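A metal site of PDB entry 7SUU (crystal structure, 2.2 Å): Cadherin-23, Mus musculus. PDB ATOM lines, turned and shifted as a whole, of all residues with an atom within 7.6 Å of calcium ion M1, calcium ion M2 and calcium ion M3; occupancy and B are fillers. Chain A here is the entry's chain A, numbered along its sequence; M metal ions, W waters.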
ATOM      1  N   GLU A  25       0.905   4.238  -8.970  1.00  0.00           N
ATOM      2  CA  GLU A  25      -0.209   4.308  -8.005  1.00  0.00           C
ATOM      3  C   GLU A  25      -0.233   2.999  -7.172  1.00  0.00           C
ATOM      4  O   GLU A  25       0.426   2.009  -7.572  1.00  0.00           O
ATOM      5  CB  GLU A  25      -1.528   4.576  -8.744  1.00  0.00           C
ATOM      6  CG  GLU A  25      -1.993   3.412  -9.581  1.00  0.00           C
ATOM      7  CD  GLU A  25      -3.452   3.426  -9.970  1.00  0.00           C
ATOM      8  OE1 GLU A  25      -3.712   3.026 -11.084  1.00  0.00           O
ATOM      9  OE2 GLU A  25      -4.315   3.801  -9.135  1.00  0.00           O
ATOM     10  N   GLU A  26      -0.943   3.015  -6.046  1.00  0.00           N
ATOM     11  CA  GLU A  26      -1.265   1.842  -5.183  1.00  0.00           C
ATOM     12  C   GLU A  26       0.002   1.210  -4.576  1.00  0.00           C
ATOM     13  O   GLU A  26      -0.080   0.075  -4.076  1.00  0.00           O
ATOM     14  CB  GLU A  26      -2.072   0.794  -5.970  1.00  0.00           C
ATOM     15  CG  GLU A  26      -3.379   1.328  -6.571  1.00  0.00           C
ATOM     16  CD  GLU A  26      -4.449   1.868  -5.634  1.00  0.00           C
ATOM     17  OE1 GLU A  26      -4.250   1.849  -4.401  1.00  0.00           O
ATOM     18  OE2 GLU A  26      -5.514   2.326  -6.146  1.00  0.00           O
ATOM     19  N   ARG A  79      -2.975   5.663   1.127  1.00  0.00           N
ATOM     20  CA  ARG A  79      -3.224   5.021  -0.167  1.00  0.00           C
ATOM     21  C   ARG A  79      -3.088   6.094  -1.240  1.00  0.00           C
ATOM     22  O   ARG A  79      -3.623   7.190  -1.037  1.00  0.00           O
ATOM     23  CB  ARG A  79      -4.641   4.451  -0.238  1.00  0.00           C
ATOM     24  CG  ARG A  79      -4.880   3.705  -1.539  1.00  0.00           C
ATOM     25  CD  ARG A  79      -6.277   3.137  -1.596  1.00  0.00           C
ATOM     26  NE  ARG A  79      -6.493   2.519  -2.895  1.00  0.00           N
ATOM     27  CZ  ARG A  79      -7.691   2.185  -3.370  1.00  0.00           C
ATOM     28  NH1 ARG A  79      -7.785   1.607  -4.563  1.00  0.00           N
ATOM     29  NH2 ARG A  79      -8.758   2.396  -2.646  1.00  0.00           N
ATOM     30  N   LEU A  80      -2.418   5.759  -2.350  1.00  0.00           N
ATOM     31  CA  LEU A  80      -2.306   6.653  -3.529  1.00  0.00           C
ATOM     32  C   LEU A  80      -3.050   6.000  -4.690  1.00  0.00           C
ATOM     33  O   LEU A  80      -2.477   5.127  -5.331  1.00  0.00           O
ATOM     34  CB  LEU A  80      -0.822   6.895  -3.845  1.00  0.00           C
ATOM     35  CG  LEU A  80      -0.084   7.784  -2.843  1.00  0.00           C
ATOM     36  CD1 LEU A  80       1.413   7.747  -3.100  1.00  0.00           C
ATOM     37  CD2 LEU A  80      -0.584   9.220  -2.906  1.00  0.00           C
ATOM     38  N   ASP A  81      -4.257   6.484  -4.969  1.00  0.00           N
ATOM     39  CA  ASP A  81      -5.184   5.943  -5.986  1.00  0.00           C
ATOM     40  C   ASP A  81      -5.312   6.974  -7.107  1.00  0.00           C
ATOM     41  O   ASP A  81      -5.870   8.051  -6.834  1.00  0.00           O
ATOM     42  CB  ASP A  81      -6.551   5.602  -5.368  1.00  0.00           C
ATOM     43  CG  ASP A  81      -7.508   4.953  -6.362  1.00  0.00           C
ATOM     44  OD1 ASP A  81      -7.081   4.599  -7.467  1.00  0.00           O
ATOM     45  OD2 ASP A  81      -8.690   4.834  -6.016  1.00  0.00           O
ATOM     46  N   ARG A  82      -4.820   6.644  -8.311  1.00  0.00           N
ATOM     47  CA  ARG A  82      -4.775   7.589  -9.450  1.00  0.00           C
ATOM     48  C   ARG A  82      -6.218   7.885  -9.833  1.00  0.00           C
ATOM     49  O   ARG A  82      -6.469   9.012 -10.244  1.00  0.00           O
ATOM     50  CB  ARG A  82      -3.984   7.022 -10.641  1.00  0.00           C
ATOM     51  CG  ARG A  82      -3.859   7.953 -11.843  1.00  0.00           C
ATOM     52  CD  ARG A  82      -3.676   7.199 -13.166  1.00  0.00           C
ATOM     53  NE  ARG A  82      -4.927   6.528 -13.504  1.00  0.00           N
ATOM     54  CZ  ARG A  82      -5.979   7.120 -14.060  1.00  0.00           C
ATOM     55  NH1 ARG A  82      -7.092   6.444 -14.260  1.00  0.00           N
ATOM     56  NH2 ARG A  82      -5.916   8.395 -14.423  1.00  0.00           N
ATOM     57  N   GLU A  83      -7.114   6.914  -9.647  1.00  0.00           N
ATOM     58  CA  GLU A  83      -8.562   7.061  -9.948  1.00  0.00           C
ATOM     59  C   GLU A  83      -9.219   7.967  -8.909  1.00  0.00           C
ATOM     60  O   GLU A  83     -10.313   8.469  -9.192  1.00  0.00           O
ATOM     61  CB  GLU A  83      -9.249   5.691 -10.040  1.00  0.00           C
ATOM     62  CG  GLU A  83      -8.915   4.943 -11.335  1.00  0.00           C
ATOM     63  CD  GLU A  83      -7.599   4.166 -11.392  1.00  0.00           C
ATOM     64  OE1 GLU A  83      -7.224   3.504 -10.408  1.00  0.00           O
ATOM     65  OE2 GLU A  83      -6.945   4.218 -12.431  1.00  0.00           O
ATOM     66  N   LYS A  84      -8.594   8.189  -7.751  1.00  0.00           N
ATOM     67  CA  LYS A  84      -9.091   9.192  -6.769  1.00  0.00           C
ATOM     68  C   LYS A  84      -8.467  10.557  -7.103  1.00  0.00           C
ATOM     69  O   LYS A  84      -9.227  11.541  -7.323  1.00  0.00           O
ATOM     70  CB  LYS A  84      -8.729   8.792  -5.341  1.00  0.00           C
ATOM     71  CG  LYS A  84      -9.401   9.642  -4.268  1.00  0.00           C
ATOM     72  CD  LYS A  84      -9.029   9.243  -2.863  1.00  0.00           C
ATOM     73  CE  LYS A  84      -9.559  10.216  -1.831  1.00  0.00           C
ATOM     74  NZ  LYS A  84      -8.668  10.280  -0.647  1.00  0.00           N
ATOM     75  N   LEU A 113       0.861  10.153 -10.501  1.00  0.00           N
ATOM     76  CA  LEU A 113       0.734   8.685 -10.364  1.00  0.00           C
ATOM     77  C   LEU A 113       0.601   8.084 -11.754  1.00  0.00           C
ATOM     78  O   LEU A 113      -0.314   8.489 -12.480  1.00  0.00           O
ATOM     79  CB  LEU A 113      -0.477   8.343  -9.507  1.00  0.00           C
ATOM     80  CG  LEU A 113      -0.468   8.902  -8.093  1.00  0.00           C
ATOM     81  CD1 LEU A 113      -1.673   8.392  -7.310  1.00  0.00           C
ATOM     82  CD2 LEU A 113       0.845   8.563  -7.390  1.00  0.00           C
ATOM     83  N   GLU A 114       1.486   7.163 -12.105  1.00  0.00           N
ATOM     84  CA  GLU A 114       1.396   6.301 -13.303  1.00  0.00           C
ATOM     85  C   GLU A 114       0.272   5.265 -13.044  1.00  0.00           C
ATOM     86  O   GLU A 114       0.192   4.688 -11.968  1.00  0.00           O
ATOM     87  CB  GLU A 114       2.806   5.745 -13.580  1.00  0.00           C
ATOM     88  CG  GLU A 114       2.823   4.467 -14.430  1.00  0.00           C
ATOM     89  CD  GLU A 114       4.176   3.832 -14.763  1.00  0.00           C
ATOM     90  OE1 GLU A 114       4.169   2.770 -15.427  1.00  0.00           O
ATOM     91  OE2 GLU A 114       5.245   4.390 -14.356  1.00  0.00           O
ATOM     92  N   ASP A 115      -0.622   5.095 -14.010  1.00  0.00           N
ATOM     93  CA  ASP A 115      -1.764   4.151 -13.944  1.00  0.00           C
ATOM     94  C   ASP A 115      -1.297   2.691 -13.876  1.00  0.00           C
ATOM     95  O   ASP A 115      -0.366   2.308 -14.614  1.00  0.00           O
ATOM     96  CB  ASP A 115      -2.641   4.336 -15.180  1.00  0.00           C
ATOM     97  CG  ASP A 115      -3.912   3.527 -15.085  1.00  0.00           C
ATOM     98  OD1 ASP A 115      -4.679   3.667 -14.049  1.00  0.00           O
ATOM     99  OD2 ASP A 115      -4.134   2.794 -16.042  1.00  0.00           O
ATOM    100  N   ILE A 116      -1.938   1.876 -13.044  1.00  0.00           N
ATOM    101  CA  ILE A 116      -1.851   0.393 -13.150  1.00  0.00           C
ATOM    102  C   ILE A 116      -3.262  -0.143 -13.437  1.00  0.00           C
ATOM    103  O   ILE A 116      -4.255   0.573 -13.144  1.00  0.00           O
ATOM    104  CB  ILE A 116      -1.248  -0.254 -11.888  1.00  0.00           C
ATOM    105  CG1 ILE A 116      -2.237  -0.204 -10.724  1.00  0.00           C
ATOM    106  CG2 ILE A 116       0.109   0.366 -11.538  1.00  0.00           C
ATOM    107  CD1 ILE A 116      -1.752  -0.929  -9.474  1.00  0.00           C
ATOM    108  N   ASP A 117      -3.314  -1.350 -13.984  1.00  0.00           N
ATOM    109  CA  ASP A 117      -4.561  -1.994 -14.436  1.00  0.00           C
ATOM    110  C   ASP A 117      -5.247  -2.579 -13.220  1.00  0.00           C
ATOM    111  O   ASP A 117      -5.150  -3.792 -13.043  1.00  0.00           O
ATOM    112  CB  ASP A 117      -4.300  -3.057 -15.499  1.00  0.00           C
ATOM    113  CG  ASP A 117      -5.561  -3.575 -16.181  1.00  0.00           C
ATOM    114  OD1 ASP A 117      -6.693  -3.050 -15.891  1.00  0.00           O
ATOM    115  OD2 ASP A 117      -5.419  -4.463 -17.020  1.00  0.00           O
ATOM    116  N   ASP A 118      -5.878  -1.754 -12.387  1.00  0.00           N
ATOM    117  CA  ASP A 118      -6.487  -2.256 -11.123  1.00  0.00           C
ATOM    118  C   ASP A 118      -7.992  -2.023 -11.146  1.00  0.00           C
ATOM    119  O   ASP A 118      -8.588  -2.097 -10.080  1.00  0.00           O
ATOM    120  CB  ASP A 118      -5.884  -1.597  -9.862  1.00  0.00           C
ATOM    121  CG  ASP A 118      -5.925  -0.070  -9.867  1.00  0.00           C
ATOM    122  OD1 ASP A 118      -6.053   0.524 -10.960  1.00  0.00           O
ATOM    123  OD2 ASP A 118      -5.808   0.510  -8.790  1.00  0.00           O
ATOM    124  N   ASN A 119      -8.584  -1.794 -12.320  1.00  0.00           N
ATOM    125  CA  ASN A 119     -10.057  -1.668 -12.457  1.00  0.00           C
ATOM    126  C   ASN A 119     -10.507  -2.513 -13.636  1.00  0.00           C
ATOM    127  O   ASN A 119      -9.733  -2.678 -14.579  1.00  0.00           O
ATOM    128  CB  ASN A 119     -10.483  -0.210 -12.619  1.00  0.00           C
ATOM    129  CG  ASN A 119     -10.230   0.579 -11.349  1.00  0.00           C
ATOM    130  OD1 ASN A 119      -9.109   1.022 -11.084  1.00  0.00           O
ATOM    131  ND2 ASN A 119     -11.263   0.733 -10.540  1.00  0.00           N
ATOM    132  N   GLU A 120     -11.744  -2.965 -13.616  1.00  0.00           N
ATOM    133  CA  GLU A 120     -12.317  -3.718 -14.756  1.00  0.00           C
ATOM    134  C   GLU A 120     -13.511  -2.928 -15.266  1.00  0.00           C
ATOM    135  O   GLU A 120     -14.080  -2.102 -14.536  1.00  0.00           O
ATOM    136  CB  GLU A 120     -12.705  -5.134 -14.355  1.00  0.00           C
ATOM    137  CG  GLU A 120     -13.781  -5.186 -13.300  1.00  0.00           C
ATOM    138  CD  GLU A 120     -14.079  -6.579 -12.744  1.00  0.00           C
ATOM    139  OE1 GLU A 120     -14.997  -6.692 -11.908  1.00  0.00           O
ATOM    140  OE2 GLU A 120     -13.408  -7.545 -13.164  1.00  0.00           O
ATOM    141  N   PRO A 121     -13.936  -3.186 -16.540  1.00  0.00           N
ATOM    142  CA  PRO A 121     -15.183  -2.633 -17.065  1.00  0.00           C
ATOM    143  C   PRO A 121     -16.373  -2.968 -16.167  1.00  0.00           C
ATOM    144  O   PRO A 121     -16.555  -4.124 -15.842  1.00  0.00           O
ATOM    145  CB  PRO A 121     -15.312  -3.296 -18.435  1.00  0.00           C
ATOM    146  CG  PRO A 121     -13.918  -3.606 -18.829  1.00  0.00           C
ATOM    147  CD  PRO A 121     -13.211  -3.995 -17.535  1.00  0.00           C
ATOM    148  N   ASP A 156     -14.141   1.446 -17.901  1.00  0.00           N
ATOM    149  CA  ASP A 156     -12.948   1.015 -17.135  1.00  0.00           C
ATOM    150  C   ASP A 156     -12.236   2.283 -16.653  1.00  0.00           C
ATOM    151  O   ASP A 156     -11.817   3.094 -17.505  1.00  0.00           O
ATOM    152  CB  ASP A 156     -12.062   0.117 -17.996  1.00  0.00           C
ATOM    153  CG  ASP A 156     -10.902  -0.582 -17.310  1.00  0.00           C
ATOM    154  OD1 ASP A 156     -10.141   0.071 -16.590  1.00  0.00           O
ATOM    155  OD2 ASP A 156     -10.706  -1.778 -17.592  1.00  0.00           O
ATOM    156  N   ALA A 157     -12.054   2.419 -15.345  1.00  0.00           N
ATOM    157  CA  ALA A 157     -11.569   3.665 -14.692  1.00  0.00           C
ATOM    158  C   ALA A 157     -10.062   3.844 -14.916  1.00  0.00           C
ATOM    159  O   ALA A 157      -9.530   4.900 -14.526  1.00  0.00           O
ATOM    160  CB  ALA A 157     -11.943   3.679 -13.220  1.00  0.00           C
ATOM    161  N   ASP A 158      -9.399   2.866 -15.535  1.00  0.00           N
ATOM    162  CA  ASP A 158      -7.925   2.904 -15.757  1.00  0.00           C
ATOM    163  C   ASP A 158      -7.633   3.794 -16.973  1.00  0.00           C
ATOM    164  O   ASP A 158      -8.501   4.553 -17.347  1.00  0.00           O
ATOM    165  CB  ASP A 158      -7.351   1.490 -15.865  1.00  0.00           C
ATOM    166  CG  ASP A 158      -7.425   0.689 -14.575  1.00  0.00           C
ATOM    167  OD1 ASP A 158      -7.298   1.279 -13.479  1.00  0.00           O
ATOM    168  OD2 ASP A 158      -7.653  -0.492 -14.665  1.00  0.00           O
ATOM    169  N   GLU A 159      -6.436   3.712 -17.544  1.00  0.00           N
ATOM    170  CA  GLU A 159      -5.941   4.655 -18.591  1.00  0.00           C
ATOM    171  C   GLU A 159      -5.458   3.896 -19.834  1.00  0.00           C
ATOM    172  O   GLU A 159      -4.781   2.871 -19.706  1.00  0.00           O
ATOM    173  CB  GLU A 159      -4.791   5.469 -18.000  1.00  0.00           C
ATOM    174  CG  GLU A 159      -4.521   6.749 -18.727  1.00  0.00           C
ATOM    175  CD  GLU A 159      -5.417   7.888 -18.307  1.00  0.00           C
ATOM    176  OE1 GLU A 159      -6.663   7.687 -18.174  1.00  0.00           O
ATOM    177  OE2 GLU A 159      -4.868   8.976 -18.098  1.00  0.00           O
ATOM    178  N   GLY A 160      -5.782   4.418 -21.013  1.00  0.00           N
ATOM    179  CA  GLY A 160      -5.235   3.920 -22.297  1.00  0.00           C
ATOM    180  C   GLY A 160      -5.383   2.401 -22.373  1.00  0.00           C
ATOM    181  O   GLY A 160      -6.488   1.880 -22.209  1.00  0.00           O
ATOM    182  N   PRO A 161      -4.284   1.645 -22.600  1.00  0.00           N
ATOM    183  CA  PRO A 161      -4.392   0.205 -22.837  1.00  0.00           C
ATOM    184  C   PRO A 161      -4.820  -0.621 -21.613  1.00  0.00           C
ATOM    185  O   PRO A 161      -5.036  -1.800 -21.761  1.00  0.00           O
ATOM    186  CB  PRO A 161      -3.006  -0.213 -23.360  1.00  0.00           C
ATOM    187  CG  PRO A 161      -2.065   0.919 -22.938  1.00  0.00           C
ATOM    188  CD  PRO A 161      -2.917   2.170 -22.765  1.00  0.00           C
ATOM    189  N   ASN A 162      -4.971   0.009 -20.452  1.00  0.00           N
ATOM    190  CA  ASN A 162      -5.492  -0.623 -19.219  1.00  0.00           C
ATOM    191  C   ASN A 162      -7.016  -0.480 -19.157  1.00  0.00           C
ATOM    192  O   ASN A 162      -7.618  -1.072 -18.250  1.00  0.00           O
ATOM    193  CB  ASN A 162      -4.873  -0.010 -17.962  1.00  0.00           C
ATOM    194  CG  ASN A 162      -3.372  -0.165 -17.913  1.00  0.00           C
ATOM    195  OD1 ASN A 162      -2.844  -1.168 -18.367  1.00  0.00           O
ATOM    196  ND2 ASN A 162      -2.687   0.825 -17.351  1.00  0.00           N
ATOM    197  N   ALA A 163      -7.627   0.244 -20.096  1.00  0.00           N
ATOM    198  CA  ALA A 163      -9.048   0.640 -20.031  1.00  0.00           C
ATOM    199  C   ALA A 163      -9.793   0.183 -21.291  1.00  0.00           C
ATOM    200  O   ALA A 163     -10.793   0.823 -21.632  1.00  0.00           O
ATOM    201  CB  ALA A 163      -9.144   2.135 -19.869  1.00  0.00           C
ATOM    202  N   ILE A 164      -9.349  -0.892 -21.954  1.00  0.00           N
ATOM    203  CA  ILE A 164     -10.058  -1.394 -23.168  1.00  0.00           C
ATOM    204  C   ILE A 164     -11.351  -2.056 -22.728  1.00  0.00           C
ATOM    205  O   ILE A 164     -11.301  -2.881 -21.838  1.00  0.00           O
ATOM    206  CB  ILE A 164      -9.168  -2.339 -23.976  1.00  0.00           C
ATOM    207  CG1 ILE A 164      -7.926  -1.590 -24.471  1.00  0.00           C
ATOM    208  CG2 ILE A 164      -9.998  -2.943 -25.110  1.00  0.00           C
ATOM    209  CD1 ILE A 164      -6.783  -2.466 -24.939  1.00  0.00           C
ATOM    210  N   SER A 208     -12.228  -6.606 -20.477  1.00  0.00           N
ATOM    211  CA  SER A 208     -10.991  -6.156 -21.154  1.00  0.00           C
ATOM    212  C   SER A 208     -10.363  -7.330 -21.891  1.00  0.00           C
ATOM    213  O   SER A 208      -9.445  -7.091 -22.682  1.00  0.00           O
ATOM    214  CB  SER A 208     -10.031  -5.491 -20.185  1.00  0.00           C
ATOM    215  OG  SER A 208     -10.635  -4.307 -19.631  1.00  0.00           O
HETATM  216 CA    CA M   1      -5.603   2.335 -12.320  1.00  0.00          CA
HETATM  217 CA    CA M   2      -6.281   2.746  -8.487  1.00  0.00          CA
HETATM  218 CA    CA M   3      -8.599  -1.919 -16.449  1.00  0.00          CA
HETATM  219  O   HOH W   1      -8.968  -3.970 -17.698  1.00  0.00           O
HETATM  220  O   HOH W   2      -8.514   1.774  -8.188  1.00  0.00           O
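The side-chain carboxylate (OE2) of Glu 25 lies close to the backbone NH (N) of Arg 82. The side-chain carboxylate (OE1) of Glu 83 lies close to the side-chain amide oxygen (OD1) of Asn 119, at 3.2 Å. N of Glu 25 sits at hydrogen-bond distance from O of Glu 114 (3.1 Å). The side-chain carboxylate (OD2) of Asp 115 sits at hydrogen-bond distance from the backbone NH (N) of Glu 159 (2.9 Å). The side-chain carboxylate of Asp 81 lies within salt-bridge range of the guanidinium group of Arg 79. N of Glu 26 lies within hydrogen-bond range of O of Leu 80, 2.7 Å away. The side-chain carboxylate of Asp 115 lies within hydrogen-bond range of the side-chain amide nitrogen of Asn 162 (2.8 Å). NE of Arg 79 is in salt-bridge range of OE1 of Glu 26 (2.8 Å).
Of the 27 residues printed, 7 come within 4 Å of calcium ion M1. Along chain A the residues within 4 Å of calcium ion M1 span positions 25 to 158. The nearest printed residue that does not touch calcium ion M1 is Arg 82 (4.4 Å).
Within 4 Å of calcium ion M2: Glu 25, Glu 26, Asp 81, Glu 83 and Asp 118. Along chain A the residues within 4 Å of calcium ion M2 span positions 25 to 118.
Of the 27 residues printed, 5 come within 4 Å of calcium ion M3. Along chain A the residues within 4 Å of calcium ion M3 span positions 117 to 162.
Calcium ion M1 is bound by the side-chain carboxylate (OD1) of Asp 118 (2.3 Å), the side-chain carboxylate (OD1) of Asp 158 (2.3 Å), the side-chain carboxylate (OE2) of Glu 83 (2.3 Å), the side-chain carboxylate (OE1) of Glu 25 (2.4 Å), the backbone carbonyl oxygen (O) of Ile 116 (2.4 Å), the side-chain carboxylate (OD1) of Asp 115 (2.4 Å) and the side-chain carboxylate (OE1) of Glu 83 (2.8 Å).
Calcium ion M2 is bound by OD1 of Asp 81, at 2.3 Å. Calcium ion M2 is bound by OE1 of Glu 83 (2.3 Å). The side-chain carboxylate (OD2) of Asp 118 binds calcium ion M2, 2.3 Å away. OE2 of Glu 25 binds calcium ion M2, 2.3 Å away. Water W2 binds calcium ion M2. The side-chain carboxylate (OE2) of Glu 26 binds calcium ion M2, 2.5 Å away.
The backbone carbonyl oxygen (O) of Asn 162 is bound to calcium ion M3, 2.2 Å away. OD1 of Asp 117 binds calcium ion M3, 2.3 Å away. O of Asn 119 is bound to calcium ion M3, at 2.3 Å. OD2 of Asp 156 is bound to calcium ion M3 (2.4 Å). Calcium ion M3 is bound by water W1 (2.4 Å). The side-chain carboxylate (OD2) of Asp 158 is bound to calcium ion M3 (2.5 Å). OD1 of Asp 156 is bound to calcium ion M3 (2.5 Å). Calcium ion M3 has seven donor atoms within binding distance.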
